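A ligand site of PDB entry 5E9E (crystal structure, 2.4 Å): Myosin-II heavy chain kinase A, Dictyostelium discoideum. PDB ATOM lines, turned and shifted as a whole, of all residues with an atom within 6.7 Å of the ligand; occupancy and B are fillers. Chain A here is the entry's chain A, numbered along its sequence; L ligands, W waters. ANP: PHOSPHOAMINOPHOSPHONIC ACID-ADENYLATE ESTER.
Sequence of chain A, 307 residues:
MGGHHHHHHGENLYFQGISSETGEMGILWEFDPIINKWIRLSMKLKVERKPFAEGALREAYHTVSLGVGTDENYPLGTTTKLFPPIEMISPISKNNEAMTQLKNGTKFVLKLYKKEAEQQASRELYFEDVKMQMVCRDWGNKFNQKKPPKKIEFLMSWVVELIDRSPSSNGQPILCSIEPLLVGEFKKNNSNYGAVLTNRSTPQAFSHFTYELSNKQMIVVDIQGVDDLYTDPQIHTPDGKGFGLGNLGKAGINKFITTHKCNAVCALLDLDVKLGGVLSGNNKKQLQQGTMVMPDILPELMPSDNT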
ATOM      1  N   PHE A  52      -0.739   8.574 -13.521  1.00  0.00           N
ATOM      2  CA  PHE A  52      -1.253   7.930 -14.728  1.00  0.00           C
ATOM      3  C   PHE A  52      -0.135   7.305 -15.560  1.00  0.00           C
ATOM      4  O   PHE A  52      -0.417   6.672 -16.563  1.00  0.00           O
ATOM      5  CB  PHE A  52      -2.027   8.912 -15.595  1.00  0.00           C
ATOM      6  CG  PHE A  52      -1.163   9.921 -16.289  1.00  0.00           C
ATOM      7  CD1 PHE A  52      -0.839  11.132 -15.684  1.00  0.00           C
ATOM      8  CD2 PHE A  52      -0.689   9.677 -17.573  1.00  0.00           C
ATOM      9  CE1 PHE A  52      -0.060  12.063 -16.332  1.00  0.00           C
ATOM     10  CE2 PHE A  52       0.094  10.622 -18.239  1.00  0.00           C
ATOM     11  CZ  PHE A  52       0.416  11.805 -17.615  1.00  0.00           C
ATOM     12  N   ALA A  53       1.124   7.496 -15.157  1.00  0.00           N
ATOM     13  CA  ALA A  53       2.249   6.970 -15.910  1.00  0.00           C
ATOM     14  C   ALA A  53       3.532   7.069 -15.104  1.00  0.00           C
ATOM     15  O   ALA A  53       3.578   7.741 -14.076  1.00  0.00           O
ATOM     16  CB  ALA A  53       2.403   7.700 -17.234  1.00  0.00           C
ATOM     17  N   GLU A  54       4.568   6.374 -15.548  1.00  0.00           N
ATOM     18  CA  GLU A  54       5.841   6.449 -14.879  1.00  0.00           C
ATOM     19  C   GLU A  54       6.985   6.113 -15.808  1.00  0.00           C
ATOM     20  O   GLU A  54       6.791   5.564 -16.886  1.00  0.00           O
ATOM     21  CB  GLU A  54       5.878   5.527 -13.661  1.00  0.00           C
ATOM     22  CG  GLU A  54       5.958   4.040 -13.970  1.00  0.00           C
ATOM     23  CD  GLU A  54       6.128   3.221 -12.725  1.00  0.00           C
ATOM     24  OE1 GLU A  54       5.108   2.664 -12.257  1.00  0.00           O
ATOM     25  OE2 GLU A  54       7.273   3.143 -12.203  1.00  0.00           O
ATOM     26  N   GLY A  55       8.179   6.464 -15.371  1.00  0.00           N
ATOM     27  CA  GLY A  55       9.399   6.122 -16.070  1.00  0.00           C
ATOM     28  C   GLY A  55      10.386   5.521 -15.101  1.00  0.00           C
ATOM     29  O   GLY A  55       9.989   5.025 -14.034  1.00  0.00           O
ATOM     30  N   ALA A  56      11.669   5.566 -15.457  1.00  0.00           N
ATOM     31  CA  ALA A  56      12.702   5.005 -14.612  1.00  0.00           C
ATOM     32  C   ALA A  56      12.751   5.706 -13.247  1.00  0.00           C
ATOM     33  O   ALA A  56      12.699   5.040 -12.213  1.00  0.00           O
ATOM     34  CB  ALA A  56      14.054   5.093 -15.307  1.00  0.00           C
ATOM     35  N   LEU A  57      12.797   7.037 -13.251  1.00  0.00           N
ATOM     36  CA  LEU A  57      12.977   7.810 -12.000  1.00  0.00           C
ATOM     37  C   LEU A  57      11.730   8.530 -11.460  1.00  0.00           C
ATOM     38  O   LEU A  57      11.669   8.814 -10.276  1.00  0.00           O
ATOM     39  CB  LEU A  57      14.129   8.811 -12.133  1.00  0.00           C
ATOM     40  CG  LEU A  57      15.481   8.205 -12.528  1.00  0.00           C
ATOM     41  CD1 LEU A  57      16.427   9.253 -13.090  1.00  0.00           C
ATOM     42  CD2 LEU A  57      16.115   7.484 -11.343  1.00  0.00           C
ATOM     43  N   ARG A  58      10.730   8.803 -12.298  1.00  0.00           N
ATOM     44  CA  ARG A  58       9.592   9.627 -11.888  1.00  0.00           C
ATOM     45  C   ARG A  58       8.214   9.057 -12.201  1.00  0.00           C
ATOM     46  O   ARG A  58       8.063   8.252 -13.123  1.00  0.00           O
ATOM     47  CB  ARG A  58       9.697  11.025 -12.510  1.00  0.00           C
ATOM     48  CG  ARG A  58      10.910  11.821 -12.053  1.00  0.00           C
ATOM     49  CD  ARG A  58      10.966  13.183 -12.698  1.00  0.00           C
ATOM     50  NE  ARG A  58      11.123  13.113 -14.153  1.00  0.00           N
ATOM     51  CZ  ARG A  58      11.046  14.156 -14.978  1.00  0.00           C
ATOM     52  NH1 ARG A  58      10.793  15.384 -14.510  1.00  0.00           N
ATOM     53  NH2 ARG A  58      11.215  13.990 -16.292  1.00  0.00           N
ATOM     54  N   GLU A  59       7.220   9.507 -11.430  1.00  0.00           N
ATOM     55  CA  GLU A  59       5.797   9.281 -11.738  1.00  0.00           C
ATOM     56  C   GLU A  59       5.129  10.589 -12.160  1.00  0.00           C
ATOM     57  O   GLU A  59       5.483  11.686 -11.707  1.00  0.00           O
ATOM     58  CB  GLU A  59       5.068   8.758 -10.506  1.00  0.00           C
ATOM     59  CG  GLU A  59       5.489   7.373 -10.059  1.00  0.00           C
ATOM     60  CD  GLU A  59       5.283   7.162  -8.565  1.00  0.00           C
ATOM     61  OE1 GLU A  59       4.612   7.983  -7.916  1.00  0.00           O
ATOM     62  OE2 GLU A  59       5.807   6.165  -8.037  1.00  0.00           O
ATOM     63  N   ALA A  60       4.127  10.462 -13.012  1.00  0.00           N
ATOM     64  CA  ALA A  60       3.459  11.603 -13.595  1.00  0.00           C
ATOM     65  C   ALA A  60       1.991  11.553 -13.206  1.00  0.00           C
ATOM     66  O   ALA A  60       1.380  10.489 -13.249  1.00  0.00           O
ATOM     67  CB  ALA A  60       3.613  11.558 -15.102  1.00  0.00           C
ATOM     68  N   HIS A  62      -1.982  13.516 -13.538  1.00  0.00           N
ATOM     69  CA  HIS A  62      -2.850  14.526 -14.133  1.00  0.00           C
ATOM     70  C   HIS A  62      -3.149  15.567 -13.076  1.00  0.00           C
ATOM     71  O   HIS A  62      -3.323  15.260 -11.899  1.00  0.00           O
ATOM     72  CB  HIS A  62      -4.151  13.927 -14.694  1.00  0.00           C
ATOM     73  CG  HIS A  62      -3.996  13.217 -16.006  1.00  0.00           C
ATOM     74  ND1 HIS A  62      -3.857  11.843 -16.112  1.00  0.00           N
ATOM     75  CD2 HIS A  62      -3.969  13.687 -17.276  1.00  0.00           C
ATOM     76  CE1 HIS A  62      -3.749  11.501 -17.383  1.00  0.00           C
ATOM     77  NE2 HIS A  62      -3.816  12.608 -18.114  1.00  0.00           N
ATOM     78  N   VAL A 109       0.578  18.192 -16.419  1.00  0.00           N
ATOM     79  CA  VAL A 109       1.222  17.059 -15.783  1.00  0.00           C
ATOM     80  C   VAL A 109       2.144  17.529 -14.679  1.00  0.00           C
ATOM     81  O   VAL A 109       2.843  18.527 -14.824  1.00  0.00           O
ATOM     82  CB  VAL A 109       2.021  16.213 -16.815  1.00  0.00           C
ATOM     83  CG1 VAL A 109       2.775  15.089 -16.135  1.00  0.00           C
ATOM     84  CG2 VAL A 109       1.066  15.623 -17.842  1.00  0.00           C
ATOM     85  N   LYS A 111       5.157  15.952 -12.112  1.00  0.00           N
ATOM     86  CA  LYS A 111       6.062  14.852 -11.973  1.00  0.00           C
ATOM     87  C   LYS A 111       6.792  14.879 -10.656  1.00  0.00           C
ATOM     88  O   LYS A 111       7.418  15.879 -10.307  1.00  0.00           O
ATOM     89  CB  LYS A 111       7.057  14.833 -13.140  1.00  0.00           C
ATOM     90  CG  LYS A 111       6.392  14.534 -14.476  1.00  0.00           C
ATOM     91  CD  LYS A 111       7.364  14.618 -15.653  1.00  0.00           C
ATOM     92  CE  LYS A 111       6.665  14.317 -16.965  1.00  0.00           C
ATOM     93  NZ  LYS A 111       7.621  14.280 -18.114  1.00  0.00           N
ATOM     94  N   TYR A 113       9.594  12.644  -8.177  1.00  0.00           N
ATOM     95  CA  TYR A 113      10.560  11.566  -8.134  1.00  0.00           C
ATOM     96  C   TYR A 113      10.001  10.448  -7.244  1.00  0.00           C
ATOM     97  O   TYR A 113       9.279  10.706  -6.292  1.00  0.00           O
ATOM     98  CB  TYR A 113      11.904  12.034  -7.585  1.00  0.00           C
ATOM     99  CG  TYR A 113      12.788  12.695  -8.624  1.00  0.00           C
ATOM    100  CD1 TYR A 113      13.526  11.936  -9.514  1.00  0.00           C
ATOM    101  CD2 TYR A 113      12.891  14.078  -8.702  1.00  0.00           C
ATOM    102  CE1 TYR A 113      14.340  12.545 -10.473  1.00  0.00           C
ATOM    103  CE2 TYR A 113      13.698  14.701  -9.645  1.00  0.00           C
ATOM    104  CZ  TYR A 113      14.427  13.920 -10.538  1.00  0.00           C
ATOM    105  OH  TYR A 113      15.241  14.536 -11.484  1.00  0.00           O
ATOM    106  N   LYS A 114      10.320   9.212  -7.609  1.00  0.00           N
ATOM    107  CA  LYS A 114       9.992   8.044  -6.789  1.00  0.00           C
ATOM    108  C   LYS A 114      11.053   7.966  -5.701  1.00  0.00           C
ATOM    109  O   LYS A 114      12.212   8.341  -5.920  1.00  0.00           O
ATOM    110  CB  LYS A 114      10.004   6.777  -7.647  1.00  0.00           C
ATOM    111  CG  LYS A 114       9.060   6.848  -8.840  1.00  0.00           C
ATOM    112  CD  LYS A 114       8.924   5.509  -9.559  1.00  0.00           C
ATOM    113  CE  LYS A 114      10.102   5.220 -10.483  1.00  0.00           C
ATOM    114  NZ  LYS A 114       9.673   4.348 -11.618  1.00  0.00           N
ATOM    115  N   LEU A 155       8.167  21.140 -24.983  1.00  0.00           N
ATOM    116  CA  LEU A 155       7.238  21.744 -24.046  1.00  0.00           C
ATOM    117  C   LEU A 155       7.982  22.553 -23.001  1.00  0.00           C
ATOM    118  O   LEU A 155       9.132  22.271 -22.674  1.00  0.00           O
ATOM    119  CB  LEU A 155       6.470  20.662 -23.323  1.00  0.00           C
ATOM    120  CG  LEU A 155       5.537  19.782 -24.139  1.00  0.00           C
ATOM    121  CD1 LEU A 155       4.951  18.756 -23.193  1.00  0.00           C
ATOM    122  CD2 LEU A 155       4.461  20.629 -24.785  1.00  0.00           C
ATOM    123  N   GLU A 179       4.532  20.357 -16.405  1.00  0.00           N
ATOM    124  CA  GLU A 179       4.604  20.628 -17.838  1.00  0.00           C
ATOM    125  C   GLU A 179       3.243  20.403 -18.472  1.00  0.00           C
ATOM    126  O   GLU A 179       2.371  19.773 -17.852  1.00  0.00           O
ATOM    127  CB  GLU A 179       5.647  19.708 -18.463  1.00  0.00           C
ATOM    128  CG  GLU A 179       5.426  18.239 -18.192  1.00  0.00           C
ATOM    129  CD  GLU A 179       6.586  17.375 -18.600  1.00  0.00           C
ATOM    130  OE1 GLU A 179       6.521  16.720 -19.666  1.00  0.00           O
ATOM    131  OE2 GLU A 179       7.567  17.321 -17.866  1.00  0.00           O
ATOM    132  N   PRO A 180       3.023  20.947 -19.690  1.00  0.00           N
ATOM    133  CA  PRO A 180       1.767  20.722 -20.386  1.00  0.00           C
ATOM    134  C   PRO A 180       1.493  19.235 -20.617  1.00  0.00           C
ATOM    135  O   PRO A 180       2.410  18.430 -20.579  1.00  0.00           O
ATOM    136  CB  PRO A 180       1.968  21.443 -21.717  1.00  0.00           C
ATOM    137  CG  PRO A 180       3.047  22.440 -21.453  1.00  0.00           C
ATOM    138  CD  PRO A 180       3.957  21.743 -20.501  1.00  0.00           C
ATOM    139  N   LEU A 181       0.225  18.879 -20.793  1.00  0.00           N
ATOM    140  CA  LEU A 181      -0.183  17.505 -21.031  1.00  0.00           C
ATOM    141  C   LEU A 181       0.014  17.191 -22.467  1.00  0.00           C
ATOM    142  O   LEU A 181      -0.482  17.927 -23.322  1.00  0.00           O
ATOM    143  CB  LEU A 181      -1.659  17.322 -20.691  1.00  0.00           C
ATOM    144  CG  LEU A 181      -2.334  15.988 -21.043  1.00  0.00           C
ATOM    145  CD1 LEU A 181      -1.710  14.834 -20.267  1.00  0.00           C
ATOM    146  CD2 LEU A 181      -3.842  16.074 -20.806  1.00  0.00           C
ATOM    147  N   LEU A 182       0.749  16.128 -22.781  1.00  0.00           N
ATOM    148  CA  LEU A 182       0.800  15.664 -24.178  1.00  0.00           C
ATOM    149  C   LEU A 182      -0.396  14.774 -24.462  1.00  0.00           C
ATOM    150  O   LEU A 182      -0.654  13.807 -23.745  1.00  0.00           O
ATOM    151  CB  LEU A 182       2.093  14.914 -24.499  1.00  0.00           C
ATOM    152  CG  LEU A 182       3.347  15.781 -24.562  1.00  0.00           C
ATOM    153  CD1 LEU A 182       4.600  14.930 -24.606  1.00  0.00           C
ATOM    154  CD2 LEU A 182       3.315  16.719 -25.748  1.00  0.00           C
ATOM    155  N   VAL A 183      -1.130  15.099 -25.520  1.00  0.00           N
ATOM    156  CA  VAL A 183      -2.252  14.266 -25.938  1.00  0.00           C
ATOM    157  C   VAL A 183      -1.875  13.450 -27.182  1.00  0.00           C
ATOM    158  O   VAL A 183      -1.688  14.001 -28.256  1.00  0.00           O
ATOM    159  CB  VAL A 183      -3.512  15.109 -26.221  1.00  0.00           C
ATOM    160  CG1 VAL A 183      -4.672  14.207 -26.639  1.00  0.00           C
ATOM    161  CG2 VAL A 183      -3.898  15.908 -24.993  1.00  0.00           C
ATOM    162  N   PHE A 186       2.597   8.442 -26.843  1.00  0.00           N
ATOM    163  CA  PHE A 186       3.873   8.941 -26.361  1.00  0.00           C
ATOM    164  C   PHE A 186       4.968   7.937 -26.715  1.00  0.00           C
ATOM    165  O   PHE A 186       4.904   6.787 -26.305  1.00  0.00           O
ATOM    166  CB  PHE A 186       3.807   9.131 -24.852  1.00  0.00           C
ATOM    167  CG  PHE A 186       4.988   9.861 -24.275  1.00  0.00           C
ATOM    168  CD1 PHE A 186       6.176   9.191 -24.053  1.00  0.00           C
ATOM    169  CD2 PHE A 186       4.886  11.185 -23.904  1.00  0.00           C
ATOM    170  CE1 PHE A 186       7.267   9.844 -23.501  1.00  0.00           C
ATOM    171  CE2 PHE A 186       5.959  11.844 -23.339  1.00  0.00           C
ATOM    172  CZ  PHE A 186       7.146  11.173 -23.141  1.00  0.00           C
ATOM    173  N   LYS A 188       9.365   7.265 -27.228  1.00  0.00           N
ATOM    174  CA  LYS A 188      10.768   7.608 -27.059  1.00  0.00           C
ATOM    175  C   LYS A 188      11.581   7.192 -28.299  1.00  0.00           C
ATOM    176  O   LYS A 188      11.579   6.027 -28.656  1.00  0.00           O
ATOM    177  CB  LYS A 188      11.304   6.946 -25.800  1.00  0.00           C
ATOM    178  CG  LYS A 188      12.771   7.239 -25.509  1.00  0.00           C
ATOM    179  CD  LYS A 188      13.089   6.862 -24.089  1.00  0.00           C
ATOM    180  CE  LYS A 188      14.529   7.141 -23.765  1.00  0.00           C
ATOM    181  NZ  LYS A 188      14.832   7.000 -22.307  1.00  0.00           N
ATOM    182  N   ASP A 222      17.543  11.699 -25.753  1.00  0.00           N
ATOM    183  CA  ASP A 222      16.293  11.380 -25.060  1.00  0.00           C
ATOM    184  C   ASP A 222      15.156  12.096 -25.767  1.00  0.00           C
ATOM    185  O   ASP A 222      14.260  12.649 -25.118  1.00  0.00           O
ATOM    186  CB  ASP A 222      16.324  11.746 -23.558  1.00  0.00           C
ATOM    187  CG  ASP A 222      16.595  10.533 -22.623  1.00  0.00           C
ATOM    188  OD1 ASP A 222      16.412   9.364 -23.051  1.00  0.00           O
ATOM    189  OD2 ASP A 222      16.982  10.768 -21.451  1.00  0.00           O
ATOM    190  N   GLN A 224      11.852  12.471 -27.116  1.00  0.00           N
ATOM    191  CA  GLN A 224      10.619  11.727 -26.853  1.00  0.00           C
ATOM    192  C   GLN A 224       9.413  12.626 -26.701  1.00  0.00           C
ATOM    193  O   GLN A 224       9.546  13.775 -26.272  1.00  0.00           O
ATOM    194  CB  GLN A 224      10.768  10.892 -25.591  1.00  0.00           C
ATOM    195  CG  GLN A 224      10.972  11.705 -24.314  1.00  0.00           C
ATOM    196  CD  GLN A 224      11.319  10.815 -23.147  1.00  0.00           C
ATOM    197  OE1 GLN A 224      10.637   9.820 -22.891  1.00  0.00           O
ATOM    198  NE2 GLN A 224      12.352  11.166 -22.423  1.00  0.00           N
ATOM    199  N   VAL A 226       5.072  13.120 -28.235  1.00  0.00           N
ATOM    200  CA  VAL A 226       3.985  12.768 -29.106  1.00  0.00           C
ATOM    201  C   VAL A 226       4.258  13.531 -30.358  1.00  0.00           C
ATOM    202  O   VAL A 226       4.263  14.760 -30.331  1.00  0.00           O
ATOM    203  CB  VAL A 226       2.602  13.160 -28.545  1.00  0.00           C
ATOM    204  CG1 VAL A 226       1.506  12.882 -29.568  1.00  0.00           C
ATOM    205  CG2 VAL A 226       2.306  12.396 -27.277  1.00  0.00           C
ATOM    206  N   THR A 231       9.374  16.267 -24.827  1.00  0.00           N
ATOM    207  CA  THR A 231       9.556  16.629 -23.431  1.00  0.00           C
ATOM    208  C   THR A 231      10.576  15.711 -22.784  1.00  0.00           C
ATOM    209  O   THR A 231      10.979  14.700 -23.351  1.00  0.00           O
ATOM    210  CB  THR A 231       8.212  16.626 -22.656  1.00  0.00           C
ATOM    211  OG1 THR A 231       8.407  17.272 -21.396  1.00  0.00           O
ATOM    212  CG2 THR A 231       7.660  15.215 -22.430  1.00  0.00           C
ATOM    213  N   ASP A 232      11.031  16.111 -21.598  1.00  0.00           N
ATOM    214  CA  ASP A 232      12.075  15.401 -20.875  1.00  0.00           C
ATOM    215  C   ASP A 232      13.259  14.908 -21.749  1.00  0.00           C
ATOM    216  O   ASP A 232      13.584  13.740 -21.758  1.00  0.00           O
ATOM    217  CB  ASP A 232      11.455  14.247 -20.085  1.00  0.00           C
ATOM    218  CG  ASP A 232      12.451  13.557 -19.183  1.00  0.00           C
ATOM    219  OD1 ASP A 232      13.323  14.245 -18.592  1.00  0.00           O
ATOM    220  OD2 ASP A 232      12.356  12.313 -19.069  1.00  0.00           O
HETATM  221  PG  ANP L   1      11.936   9.728 -15.760  1.00  0.00           P
HETATM  222  O1G ANP L   1      10.716   8.863 -15.722  1.00  0.00           O
HETATM  223  O2G ANP L   1      11.753  11.226 -15.874  1.00  0.00           O
HETATM  224  O3G ANP L   1      12.920   9.250 -14.745  1.00  0.00           O
HETATM  225  PB  ANP L   1      11.714   8.940 -18.593  1.00  0.00           P
HETATM  226  O1B ANP L   1      11.386   7.505 -18.251  1.00  0.00           O
HETATM  227  O2B ANP L   1      12.612   9.063 -19.811  1.00  0.00           O
HETATM  228  N3B ANP L   1      12.703   9.452 -17.283  1.00  0.00           N
HETATM  229  PA  ANP L   1       9.318  10.731 -17.757  1.00  0.00           P
HETATM  230  O1A ANP L   1       9.444  10.412 -16.321  1.00  0.00           O
HETATM  231  O2A ANP L   1       9.341  12.192 -18.147  1.00  0.00           O
HETATM  232  O3A ANP L   1      10.345   9.878 -18.751  1.00  0.00           O
HETATM  233  O5' ANP L   1       7.809  10.289 -18.071  1.00  0.00           O
HETATM  234  C5' ANP L   1       7.230   9.067 -17.633  1.00  0.00           C
HETATM  235  C4' ANP L   1       6.079   8.725 -18.558  1.00  0.00           C
HETATM  236  O4' ANP L   1       4.986   9.657 -18.428  1.00  0.00           O
HETATM  237  C3' ANP L   1       6.494   8.785 -20.005  1.00  0.00           C
HETATM  238  O3' ANP L   1       7.089   7.572 -20.408  1.00  0.00           O
HETATM  239  C2' ANP L   1       5.172   9.089 -20.682  1.00  0.00           C
HETATM  240  O2' ANP L   1       4.412   7.892 -20.859  1.00  0.00           O
HETATM  241  C1' ANP L   1       4.420   9.966 -19.701  1.00  0.00           C
HETATM  242  N9  ANP L   1       4.597  11.414 -19.901  1.00  0.00           N
HETATM  243  C8  ANP L   1       5.736  12.091 -19.608  1.00  0.00           C
HETATM  244  N7  ANP L   1       5.605  13.429 -19.859  1.00  0.00           N
HETATM  245  C5  ANP L   1       4.361  13.621 -20.303  1.00  0.00           C
HETATM  246  C6  ANP L   1       3.569  14.786 -20.741  1.00  0.00           C
HETATM  247  N6  ANP L   1       4.102  16.024 -20.743  1.00  0.00           N
HETATM  248  N1  ANP L   1       2.294  14.586 -21.131  1.00  0.00           N
HETATM  249  C2  ANP L   1       1.761  13.348 -21.129  1.00  0.00           C
HETATM  250  N3  ANP L   1       2.422  12.257 -20.758  1.00  0.00           N
HETATM  251  C4  ANP L   1       3.697  12.302 -20.333  1.00  0.00           C
HETATM  252  O   HOH W   1       2.112   7.941 -21.869  1.00  0.00           O
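Merely in contact with the ligand: Gly 55 (3.1 Å), Ala 53 (3.5 Å), Glu 54 (3.5 Å), Phe 186 (3.5 Å), Val 109 (3.7 Å), Leu 181 (3.7 Å), Thr 231 (3.7 Å), Phe 52 (3.8 Å) and Leu 155 (3.8 Å). Hydrophobic or aromatic side chains that line the ligand: Phe 52, Ala 53, Leu 57, Val 109, Leu 155, Leu 181, Leu 182 and Phe 186. 19 residues have an atom within 4 Å of the ligand: Phe 52, Ala 53, Glu 54, Gly 55, Ala 56, Leu 57, Arg 58, Val 109, Lys 111, Leu 155, Glu 179, Pro 180, Leu 181, Leu 182, Phe 186, Lys 188, Gln 224, Thr 231 and Asp 232. The nearest printed residue that does not touch the ligand is Ala 60 (4.1 Å).
NZ of Lys 111 lies within salt-bridge range of O2A of the ligand (2.7 Å). A nitrogen (N3B) of the ligand is in hydrogen-bond range of the side-chain carboxylate (OD2) of Asp 232 (3.4 Å). O1B of the ligand lies within hydrogen-bond range of N of Ala 56 (3.4 Å). N6 of the ligand is in hydrogen-bond range of O of Pro 180 (2.9 Å). N of Leu 57 lies within hydrogen-bond range of O3G of the ligand (2.7 Å). An oxygen (O3G) of the ligand is in hydrogen-bond range of the backbone NH of Arg 58 (3.3 Å). An oxygen (O2G) of the ligand is in salt-bridge range of the guanidinium group of Arg 58, 2.6 Å away. A nitrogen (N1) of the ligand sits at hydrogen-bond distance from the backbone NH (N) of Leu 182 (2.7 Å). NE2 of Gln 224 lies within hydrogen-bond range of O2B of the ligand (3.4 Å). O2B of the ligand lies within salt-bridge range of NZ of Lys 188. A nitrogen (N6) of the ligand is in hydrogen-bond range of the side-chain carboxylate (OE1) of Glu 179.
The backbone carbonyl oxygen (O) of Ala 56 sits close to the side-chain amino group (NZ) of Lys 114, 3.2 Å away. The side-chain carboxylate (OE1) of Glu 179 is in hydrogen-bond range of the side-chain hydroxyl (OG1) of Thr 231 (2.6 Å). The backbone carbonyl oxygen of Glu 179 sits at hydrogen-bond distance from the backbone NH of Val 109 (2.8 Å). NZ of Lys 188 is in salt-bridge range of OD1 of Asp 222, 2.9 Å away. OD1 of Asp 232 is in salt-bridge range of NH2 of Arg 58 (3.1 Å). The side-chain carboxylate (OE2) of Glu 54 lies within salt-bridge range of the side-chain amino group (NZ) of Lys 114 (2.7 Å). O of Gln 224 lies within hydrogen-bond range of N of Thr 231. The backbone carbonyl oxygen (O) of Ala 60 lies within hydrogen-bond range of the backbone NH (N) of Phe 52.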
